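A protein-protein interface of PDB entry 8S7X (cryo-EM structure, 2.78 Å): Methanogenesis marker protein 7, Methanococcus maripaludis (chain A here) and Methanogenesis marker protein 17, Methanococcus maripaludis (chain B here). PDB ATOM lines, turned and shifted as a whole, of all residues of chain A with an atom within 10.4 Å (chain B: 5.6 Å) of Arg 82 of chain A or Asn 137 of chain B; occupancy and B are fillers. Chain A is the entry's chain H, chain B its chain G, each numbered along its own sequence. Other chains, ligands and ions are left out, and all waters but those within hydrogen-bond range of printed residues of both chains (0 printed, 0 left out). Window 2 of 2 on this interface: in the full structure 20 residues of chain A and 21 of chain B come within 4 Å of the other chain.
The guanidinium group of Arg 178 of chain A sits at hydrogen-bond distance from the backbone carbonyl oxygen of Arg 138 of chain B (2.8 Å).
NH1 of Arg 178 of chain A lies within hydrogen-bond range of O of Val 139 of chain B.
The backbone carbonyl oxygen (O) of Phe 140 of chain B lies within hydrogen-bond range of a ring nitrogen (NE2) of His 83 of chain A, at 2.9 Å.
OD2 of Asp 134 of chain B lies within salt-bridge range of NH2 of Arg 138 of chain B (3.2 Å).
The guanidinium group (NH1) of Arg 147 of chain B is in hydrogen-bond range of the side-chain amide oxygen (OD1) of Asn 137 of chain B (3.4 Å).
A ring nitrogen (ND1) of His 83 of chain A is in hydrogen-bond range of the side-chain hydroxyl (OG) of Ser 81 of chain A, at 3.4 Å.
Among the printed residues, pairs that only touch across the chains: Arg 82 of chain A with Asn 137 of chain B (3.7 Å), His 83 of chain A with Asn 137 of chain B (3.8 Å) and Arg 178 of chain A with Phe 140 of chain B (3.8 Å).
Ser 77 of chain A touches none of the printed residues of chain B.
Pro 78 of chain A touches none of the printed residues of chain B.
Printed residues of chain B within 4 Å of His 83 of chain A: Asn 137 (3.8 Å) and Phe 140 (2.9 Å).
No residue of chain A comes within 4 Å of Asp 134 of chain B.
Asn 137 of chain B touches two residues of chain A.
Arg 138 of chain B touches one residue of chain A.
Of the printed residues of chain A, Val 139 of chain B touches Arg 178 (3.0 Å).
Of the printed residues of chain A, Phe 140 of chain B touches His 83 and Arg 178.
The nearest residue of chain B that does not touch Arg 82 of chain A is Arg 138 of chain B (4.2 Å).
Of the 21 printed residues of chain A, 3 touch a printed residue of chain B.
Among the printed residues, 6 pairs touch across the chains.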
ATOM      1  N   SER A  77     -26.664 -20.955  14.427  1.00  0.00           N
ATOM      2  CA  SER A  77     -26.450 -20.120  15.591  1.00  0.00           C
ATOM      3  C   SER A  77     -25.406 -19.053  15.284  1.00  0.00           C
ATOM      4  O   SER A  77     -24.479 -19.292  14.505  1.00  0.00           O
ATOM      5  CB  SER A  77     -25.988 -20.963  16.771  1.00  0.00           C
ATOM      6  OG  SER A  77     -25.004 -20.277  17.522  1.00  0.00           O
ATOM      7  N   PRO A  78     -25.537 -17.862  15.867  1.00  0.00           N
ATOM      8  CA  PRO A  78     -24.548 -16.808  15.591  1.00  0.00           C
ATOM      9  C   PRO A  78     -23.139 -17.178  16.007  1.00  0.00           C
ATOM     10  O   PRO A  78     -22.177 -16.669  15.422  1.00  0.00           O
ATOM     11  CB  PRO A  78     -25.082 -15.615  16.393  1.00  0.00           C
ATOM     12  CG  PRO A  78     -26.529 -15.890  16.549  1.00  0.00           C
ATOM     13  CD  PRO A  78     -26.646 -17.368  16.695  1.00  0.00           C
ATOM     14  N   SER A  79     -22.986 -18.043  17.002  1.00  0.00           N
ATOM     15  CA  SER A  79     -21.674 -18.501  17.433  1.00  0.00           C
ATOM     16  C   SER A  79     -21.861 -19.777  18.236  1.00  0.00           C
ATOM     17  O   SER A  79     -22.976 -20.141  18.611  1.00  0.00           O
ATOM     18  CB  SER A  79     -20.948 -17.438  18.257  1.00  0.00           C
ATOM     19  OG  SER A  79     -21.170 -17.635  19.640  1.00  0.00           O
ATOM     20  N   LEU A  80     -20.749 -20.460  18.492  1.00  0.00           N
ATOM     21  CA  LEU A  80     -20.749 -21.664  19.308  1.00  0.00           C
ATOM     22  C   LEU A  80     -20.375 -21.378  20.758  1.00  0.00           C
ATOM     23  O   LEU A  80     -20.007 -22.300  21.492  1.00  0.00           O
ATOM     24  CB  LEU A  80     -19.802 -22.704  18.714  1.00  0.00           C
ATOM     25  CG  LEU A  80     -20.199 -23.349  17.386  1.00  0.00           C
ATOM     26  CD1 LEU A  80     -19.558 -24.712  17.268  1.00  0.00           C
ATOM     27  CD2 LEU A  80     -21.705 -23.460  17.251  1.00  0.00           C
ATOM     28  N   SER A  81     -20.464 -20.122  21.184  1.00  0.00           N
ATOM     29  CA  SER A  81     -20.044 -19.728  22.516  1.00  0.00           C
ATOM     30  C   SER A  81     -21.121 -20.066  23.543  1.00  0.00           C
ATOM     31  O   SER A  81     -22.157 -20.656  23.233  1.00  0.00           O
ATOM     32  CB  SER A  81     -19.718 -18.241  22.541  1.00  0.00           C
ATOM     33  OG  SER A  81     -20.849 -17.480  22.174  1.00  0.00           O
ATOM     34  N   ARG A  82     -20.873 -19.670  24.792  1.00  0.00           N
ATOM     35  CA  ARG A  82     -21.782 -19.983  25.887  1.00  0.00           C
ATOM     36  C   ARG A  82     -23.120 -19.271  25.764  1.00  0.00           C
ATOM     37  O   ARG A  82     -24.074 -19.656  26.446  1.00  0.00           O
ATOM     38  CB  ARG A  82     -21.139 -19.612  27.221  1.00  0.00           C
ATOM     39  CG  ARG A  82     -21.182 -18.125  27.529  1.00  0.00           C
ATOM     40  CD  ARG A  82     -19.818 -17.599  27.912  1.00  0.00           C
ATOM     41  NE  ARG A  82     -19.417 -18.059  29.233  1.00  0.00           N
ATOM     42  CZ  ARG A  82     -18.173 -18.362  29.572  1.00  0.00           C
ATOM     43  NH1 ARG A  82     -17.180 -18.272  28.706  1.00  0.00           N
ATOM     44  NH2 ARG A  82     -17.921 -18.774  30.811  1.00  0.00           N
ATOM     45  N   HIS A  83     -23.210 -18.241  24.924  1.00  0.00           N
ATOM     46  CA  HIS A  83     -24.448 -17.479  24.831  1.00  0.00           C
ATOM     47  C   HIS A  83     -25.545 -18.274  24.142  1.00  0.00           C
ATOM     48  O   HIS A  83     -26.684 -18.308  24.615  1.00  0.00           O
ATOM     49  CB  HIS A  83     -24.192 -16.167  24.100  1.00  0.00           C
ATOM     50  CG  HIS A  83     -23.191 -15.294  24.777  1.00  0.00           C
ATOM     51  ND1 HIS A  83     -21.838 -15.542  24.733  1.00  0.00           N
ATOM     52  CD2 HIS A  83     -23.345 -14.181  25.529  1.00  0.00           C
ATOM     53  CE1 HIS A  83     -21.199 -14.616  25.425  1.00  0.00           C
ATOM     54  NE2 HIS A  83     -22.092 -13.778  25.918  1.00  0.00           N
ATOM     55  N   HIS A  84     -25.220 -18.930  23.035  1.00  0.00           N
ATOM     56  CA  HIS A  84     -26.218 -19.629  22.244  1.00  0.00           C
ATOM     57  C   HIS A  84     -26.070 -21.136  22.247  1.00  0.00           C
ATOM     58  O   HIS A  84     -27.082 -21.833  22.235  1.00  0.00           O
ATOM     59  CB  HIS A  84     -26.176 -19.152  20.787  1.00  0.00           C
ATOM     60  CG  HIS A  84     -25.555 -17.804  20.612  1.00  0.00           C
ATOM     61  ND1 HIS A  84     -24.193 -17.620  20.538  1.00  0.00           N
ATOM     62  CD2 HIS A  84     -26.107 -16.577  20.490  1.00  0.00           C
ATOM     63  CE1 HIS A  84     -23.934 -16.335  20.382  1.00  0.00           C
ATOM     64  NE2 HIS A  84     -25.078 -15.681  20.351  1.00  0.00           N
ATOM     65  N   LEU A  85     -24.845 -21.660  22.260  1.00  0.00           N
ATOM     66  CA  LEU A  85     -24.664 -23.091  22.009  1.00  0.00           C
ATOM     67  C   LEU A  85     -25.194 -23.958  23.145  1.00  0.00           C
ATOM     68  O   LEU A  85     -26.134 -24.738  22.916  1.00  0.00           O
ATOM     69  CB  LEU A  85     -23.196 -23.384  21.711  1.00  0.00           C
ATOM     70  CG  LEU A  85     -22.868 -24.862  21.584  1.00  0.00           C
ATOM     71  CD1 LEU A  85     -23.034 -25.319  20.147  1.00  0.00           C
ATOM     72  CD2 LEU A  85     -21.466 -25.108  22.102  1.00  0.00           C
ATOM     73  N   PRO A  86     -24.673 -23.876  24.371  1.00  0.00           N
ATOM     74  CA  PRO A  86     -25.027 -24.894  25.370  1.00  0.00           C
ATOM     75  C   PRO A  86     -26.469 -24.848  25.798  1.00  0.00           C
ATOM     76  O   PRO A  86     -26.889 -25.745  26.536  1.00  0.00           O
ATOM     77  CB  PRO A  86     -24.105 -24.573  26.551  1.00  0.00           C
ATOM     78  CG  PRO A  86     -23.289 -23.398  26.125  1.00  0.00           C
ATOM     79  CD  PRO A  86     -23.964 -22.751  24.990  1.00  0.00           C
ATOM     80  N   HIS A  87     -27.234 -23.838  25.379  1.00  0.00           N
ATOM     81  CA  HIS A  87     -28.655 -23.770  25.693  1.00  0.00           C
ATOM     82  C   HIS A  87     -29.373 -22.918  24.662  1.00  0.00           C
ATOM     83  O   HIS A  87     -28.860 -21.892  24.216  1.00  0.00           O
ATOM     84  CB  HIS A  87     -28.902 -23.237  27.103  1.00  0.00           C
ATOM     85  CG  HIS A  87     -28.893 -24.309  28.140  1.00  0.00           C
ATOM     86  ND1 HIS A  87     -29.664 -25.445  28.034  1.00  0.00           N
ATOM     87  CD2 HIS A  87     -28.183 -24.442  29.284  1.00  0.00           C
ATOM     88  CE1 HIS A  87     -29.444 -26.223  29.077  1.00  0.00           C
ATOM     89  NE2 HIS A  87     -28.551 -25.636  29.850  1.00  0.00           N
ATOM     90  N   ILE A  88     -30.597 -23.351  24.346  1.00  0.00           N
ATOM     91  CA  ILE A  88     -31.442 -22.932  23.230  1.00  0.00           C
ATOM     92  C   ILE A  88     -31.022 -23.659  21.960  1.00  0.00           C
ATOM     93  O   ILE A  88     -31.829 -24.374  21.360  1.00  0.00           O
ATOM     94  CB  ILE A  88     -31.461 -21.410  23.022  1.00  0.00           C
ATOM     95  CG1 ILE A  88     -31.934 -20.738  24.298  1.00  0.00           C
ATOM     96  CG2 ILE A  88     -32.414 -21.050  21.909  1.00  0.00           C
ATOM     97  CD1 ILE A  88     -33.274 -21.241  24.744  1.00  0.00           C
ATOM     98  N   ALA A  89     -29.768 -23.494  21.536  1.00  0.00           N
ATOM     99  CA  ALA A  89     -29.337 -24.135  20.297  1.00  0.00           C
ATOM    100  C   ALA A  89     -29.420 -25.651  20.407  1.00  0.00           C
ATOM    101  O   ALA A  89     -29.926 -26.322  19.501  1.00  0.00           O
ATOM    102  CB  ALA A  89     -27.921 -23.696  19.935  1.00  0.00           C
ATOM    103  N   CYS A  90     -28.943 -26.212  21.518  1.00  0.00           N
ATOM    104  CA  CYS A  90     -29.077 -27.649  21.717  1.00  0.00           C
ATOM    105  C   CYS A  90     -30.527 -28.044  21.877  1.00  0.00           C
ATOM    106  O   CYS A  90     -30.924 -29.130  21.459  1.00  0.00           O
ATOM    107  CB  CYS A  90     -28.317 -28.106  22.948  1.00  0.00           C
ATOM    108  SG  CYS A  90     -28.325 -26.884  24.228  1.00  0.00           S
ATOM    109  N   ASP A  91     -31.324 -27.207  22.538  1.00  0.00           N
ATOM    110  CA  ASP A  91     -32.733 -27.531  22.692  1.00  0.00           C
ATOM    111  C   ASP A  91     -33.424 -27.580  21.338  1.00  0.00           C
ATOM    112  O   ASP A  91     -34.212 -28.492  21.070  1.00  0.00           O
ATOM    113  CB  ASP A  91     -33.404 -26.526  23.620  1.00  0.00           C
ATOM    114  CG  ASP A  91     -32.656 -26.354  24.922  1.00  0.00           C
ATOM    115  OD1 ASP A  91     -31.548 -25.789  24.902  1.00  0.00           O
ATOM    116  OD2 ASP A  91     -33.168 -26.805  25.966  1.00  0.00           O
ATOM    117  N   ALA A 112     -22.357 -12.664  15.376  1.00  0.00           N
ATOM    118  CA  ALA A 112     -22.730 -11.912  16.562  1.00  0.00           C
ATOM    119  C   ALA A 112     -22.557 -10.415  16.333  1.00  0.00           C
ATOM    120  O   ALA A 112     -21.770  -9.976  15.492  1.00  0.00           O
ATOM    121  CB  ALA A 112     -21.896 -12.355  17.766  1.00  0.00           C
ATOM    122  N   GLY A 177     -35.774 -16.956  22.575  1.00  0.00           N
ATOM    123  CA  GLY A 177     -34.657 -16.052  22.479  1.00  0.00           C
ATOM    124  C   GLY A 177     -33.379 -16.681  22.977  1.00  0.00           C
ATOM    125  O   GLY A 177     -33.283 -17.897  23.179  1.00  0.00           O
ATOM    126  N   ARG A 178     -32.376 -15.839  23.179  1.00  0.00           N
ATOM    127  CA  ARG A 178     -31.136 -16.278  23.797  1.00  0.00           C
ATOM    128  C   ARG A 178     -31.376 -16.453  25.287  1.00  0.00           C
ATOM    129  O   ARG A 178     -31.649 -15.478  25.993  1.00  0.00           O
ATOM    130  CB  ARG A 178     -30.028 -15.263  23.535  1.00  0.00           C
ATOM    131  CG  ARG A 178     -28.751 -15.547  24.283  1.00  0.00           C
ATOM    132  CD  ARG A 178     -28.399 -14.403  25.199  1.00  0.00           C
ATOM    133  NE  ARG A 178     -27.453 -14.811  26.224  1.00  0.00           N
ATOM    134  CZ  ARG A 178     -26.701 -13.974  26.919  1.00  0.00           C
ATOM    135  NH1 ARG A 178     -26.767 -12.667  26.731  1.00  0.00           N
ATOM    136  NH2 ARG A 178     -25.860 -14.459  27.827  1.00  0.00           N
ATOM    137  N   ARG A 179     -31.295 -17.688  25.767  1.00  0.00           N
ATOM    138  CA  ARG A 179     -31.531 -17.988  27.168  1.00  0.00           C
ATOM    139  C   ARG A 179     -30.295 -18.655  27.755  1.00  0.00           C
ATOM    140  O   ARG A 179     -29.252 -18.767  27.104  1.00  0.00           O
ATOM    141  CB  ARG A 179     -32.770 -18.870  27.346  1.00  0.00           C
ATOM    142  CG  ARG A 179     -34.059 -18.088  27.460  1.00  0.00           C
ATOM    143  CD  ARG A 179     -34.977 -18.368  26.294  1.00  0.00           C
ATOM    144  NE  ARG A 179     -36.178 -17.544  26.333  1.00  0.00           N
ATOM    145  CZ  ARG A 179     -37.328 -17.918  26.876  1.00  0.00           C
ATOM    146  NH1 ARG A 179     -37.468 -19.095  27.460  1.00  0.00           N
ATOM    147  NH2 ARG A 179     -38.365 -17.087  26.833  1.00  0.00           N
ATOM    148  N   ALA A 180     -30.412 -19.093  29.008  1.00  0.00           N
ATOM    149  CA  ALA A 180     -29.319 -19.760  29.694  1.00  0.00           C
ATOM    150  C   ALA A 180     -29.758 -20.993  30.469  1.00  0.00           C
ATOM    151  O   ALA A 180     -28.913 -21.638  31.096  1.00  0.00           O
ATOM    152  CB  ALA A 180     -28.608 -18.786  30.643  1.00  0.00           C
ATOM    153  N   GLN A 181     -31.038 -21.334  30.450  1.00  0.00           N
ATOM    154  CA  GLN A 181     -31.551 -22.526  31.102  1.00  0.00           C
ATOM    155  C   GLN A 181     -32.054 -23.514  30.062  1.00  0.00           C
ATOM    156  O   GLN A 181     -32.277 -23.170  28.902  1.00  0.00           O
ATOM    157  CB  GLN A 181     -32.689 -22.194  32.066  1.00  0.00           C
ATOM    158  CG  GLN A 181     -32.338 -21.203  33.133  1.00  0.00           C
ATOM    159  CD  GLN A 181     -32.509 -21.768  34.524  1.00  0.00           C
ATOM    160  OE1 GLN A 181     -32.692 -21.029  35.490  1.00  0.00           O
ATOM    161  NE2 GLN A 181     -32.459 -23.090  34.634  1.00  0.00           N
ATOM    162  N   VAL B 132     -17.325 -11.553  39.906  1.00  0.00           N
ATOM    163  CA  VAL B 132     -18.210 -10.520  39.382  1.00  0.00           C
ATOM    164  C   VAL B 132     -17.941 -10.270  37.900  1.00  0.00           C
ATOM    165  O   VAL B 132     -18.877 -10.120  37.105  1.00  0.00           O
ATOM    166  CB  VAL B 132     -18.082  -9.236  40.218  1.00  0.00           C
ATOM    167  CG1 VAL B 132     -18.791  -8.095  39.539  1.00  0.00           C
ATOM    168  CG2 VAL B 132     -18.662  -9.458  41.600  1.00  0.00           C
ATOM    169  N   LEU B 133     -16.667 -10.207  37.500  1.00  0.00           N
ATOM    170  CA  LEU B 133     -16.396 -10.045  36.071  1.00  0.00           C
ATOM    171  C   LEU B 133     -16.826 -11.268  35.277  1.00  0.00           C
ATOM    172  O   LEU B 133     -17.226 -11.139  34.114  1.00  0.00           O
ATOM    173  CB  LEU B 133     -14.926  -9.735  35.764  1.00  0.00           C
ATOM    174  CG  LEU B 133     -14.138  -8.526  36.293  1.00  0.00           C
ATOM    175  CD1 LEU B 133     -15.011  -7.272  36.381  1.00  0.00           C
ATOM    176  CD2 LEU B 133     -13.307  -8.759  37.536  1.00  0.00           C
ATOM    177  N   ASP B 134     -16.757 -12.457  35.872  1.00  0.00           N
ATOM    178  CA  ASP B 134     -17.314 -13.628  35.207  1.00  0.00           C
ATOM    179  C   ASP B 134     -18.811 -13.462  34.984  1.00  0.00           C
ATOM    180  O   ASP B 134     -19.335 -13.822  33.924  1.00  0.00           O
ATOM    181  CB  ASP B 134     -17.023 -14.884  36.021  1.00  0.00           C
ATOM    182  CG  ASP B 134     -17.217 -16.151  35.220  1.00  0.00           C
ATOM    183  OD1 ASP B 134     -17.206 -16.077  33.974  1.00  0.00           O
ATOM    184  OD2 ASP B 134     -17.382 -17.223  35.834  1.00  0.00           O
ATOM    185  N   PHE B 135     -19.512 -12.913  35.978  1.00  0.00           N
ATOM    186  CA  PHE B 135     -20.940 -12.646  35.829  1.00  0.00           C
ATOM    187  C   PHE B 135     -21.209 -11.654  34.702  1.00  0.00           C
ATOM    188  O   PHE B 135     -22.118 -11.861  33.885  1.00  0.00           O
ATOM    189  CB  PHE B 135     -21.503 -12.137  37.159  1.00  0.00           C
ATOM    190  CG  PHE B 135     -22.842 -11.473  37.047  1.00  0.00           C
ATOM    191  CD1 PHE B 135     -24.002 -12.224  37.066  1.00  0.00           C
ATOM    192  CD2 PHE B 135     -22.945 -10.099  36.949  1.00  0.00           C
ATOM    193  CE1 PHE B 135     -25.232 -11.618  36.972  1.00  0.00           C
ATOM    194  CE2 PHE B 135     -24.173  -9.490  36.852  1.00  0.00           C
ATOM    195  CZ  PHE B 135     -25.318 -10.250  36.864  1.00  0.00           C
ATOM    196  N   MET B 136     -20.432 -10.570  34.636  1.00  0.00           N
ATOM    197  CA  MET B 136     -20.578  -9.631  33.522  1.00  0.00           C
ATOM    198  C   MET B 136     -20.336 -10.306  32.179  1.00  0.00           C
ATOM    199  O   MET B 136     -21.064 -10.051  31.213  1.00  0.00           O
ATOM    200  CB  MET B 136     -19.635  -8.432  33.662  1.00  0.00           C
ATOM    201  CG  MET B 136     -19.403  -7.886  35.045  1.00  0.00           C
ATOM    202  SD  MET B 136     -20.458  -6.442  35.268  1.00  0.00           S
ATOM    203  CE  MET B 136     -20.469  -6.286  37.041  1.00  0.00           C
ATOM    204  N   ASN B 137     -19.308 -11.148  32.093  1.00  0.00           N
ATOM    205  CA  ASN B 137     -19.025 -11.832  30.834  1.00  0.00           C
ATOM    206  C   ASN B 137     -20.173 -12.748  30.439  1.00  0.00           C
ATOM    207  O   ASN B 137     -20.506 -12.862  29.254  1.00  0.00           O
ATOM    208  CB  ASN B 137     -17.726 -12.624  30.949  1.00  0.00           C
ATOM    209  CG  ASN B 137     -17.445 -13.455  29.717  1.00  0.00           C
ATOM    210  OD1 ASN B 137     -17.469 -12.952  28.596  1.00  0.00           O
ATOM    211  ND2 ASN B 137     -17.183 -14.739  29.918  1.00  0.00           N
ATOM    212  N   ARG B 138     -20.780 -13.421  31.417  1.00  0.00           N
ATOM    213  CA  ARG B 138     -21.898 -14.310  31.118  1.00  0.00           C
ATOM    214  C   ARG B 138     -23.119 -13.536  30.640  1.00  0.00           C
ATOM    215  O   ARG B 138     -23.748 -13.916  29.646  1.00  0.00           O
ATOM    216  CB  ARG B 138     -22.246 -15.141  32.347  1.00  0.00           C
ATOM    217  CG  ARG B 138     -21.416 -16.392  32.505  1.00  0.00           C
ATOM    218  CD  ARG B 138     -21.819 -17.158  33.745  1.00  0.00           C
ATOM    219  NE  ARG B 138     -20.675 -17.809  34.371  1.00  0.00           N
ATOM    220  CZ  ARG B 138     -20.661 -19.069  34.780  1.00  0.00           C
ATOM    221  NH1 ARG B 138     -21.719 -19.851  34.640  1.00  0.00           N
ATOM    222  NH2 ARG B 138     -19.561 -19.556  35.341  1.00  0.00           N
ATOM    223  N   VAL B 139     -23.482 -12.455  31.334  1.00  0.00           N
ATOM    224  CA  VAL B 139     -24.742 -11.779  31.035  1.00  0.00           C
ATOM    225  C   VAL B 139     -24.662 -10.988  29.734  1.00  0.00           C
ATOM    226  O   VAL B 139     -25.601 -11.000  28.933  1.00  0.00           O
ATOM    227  CB  VAL B 139     -25.160 -10.884  32.213  1.00  0.00           C
ATOM    228  CG1 VAL B 139     -26.384 -10.073  31.849  1.00  0.00           C
ATOM    229  CG2 VAL B 139     -25.443 -11.730  33.432  1.00  0.00           C
ATOM    230  N   PHE B 140     -23.552 -10.297  29.500  1.00  0.00           N
ATOM    231  CA  PHE B 140     -23.467  -9.373  28.381  1.00  0.00           C
ATOM    232  C   PHE B 140     -23.644 -10.105  27.053  1.00  0.00           C
ATOM    233  O   PHE B 140     -23.213 -11.252  26.902  1.00  0.00           O
ATOM    234  CB  PHE B 140     -22.122  -8.655  28.390  1.00  0.00           C
ATOM    235  CG  PHE B 140     -22.141  -7.328  29.087  1.00  0.00           C
ATOM    236  CD1 PHE B 140     -23.063  -6.364  28.741  1.00  0.00           C
ATOM    237  CD2 PHE B 140     -21.222  -7.045  30.078  1.00  0.00           C
ATOM    238  CE1 PHE B 140     -23.073  -5.148  29.380  1.00  0.00           C
ATOM    239  CE2 PHE B 140     -21.230  -5.828  30.715  1.00  0.00           C
ATOM    240  CZ  PHE B 140     -22.155  -4.879  30.365  1.00  0.00           C
ATOM    241  N   ARG B 147     -15.402  -3.369  26.282  1.00  0.00           N
ATOM    242  CA  ARG B 147     -15.921  -3.181  27.626  1.00  0.00           C
ATOM    243  C   ARG B 147     -14.906  -2.432  28.478  1.00  0.00           C
ATOM    244  O   ARG B 147     -13.695  -2.576  28.300  1.00  0.00           O
ATOM    245  CB  ARG B 147     -16.257  -4.525  28.290  1.00  0.00           C
ATOM    246  CG  ARG B 147     -17.125  -5.435  27.442  1.00  0.00           C
ATOM    247  CD  ARG B 147     -17.399  -6.750  28.137  1.00  0.00           C
ATOM    248  NE  ARG B 147     -18.302  -7.588  27.359  1.00  0.00           N
ATOM    249  CZ  ARG B 147     -18.495  -8.882  27.573  1.00  0.00           C
ATOM    250  NH1 ARG B 147     -17.856  -9.526  28.533  1.00  0.00           N
ATOM    251  NH2 ARG B 147     -19.354  -9.545  26.802  1.00  0.00           N
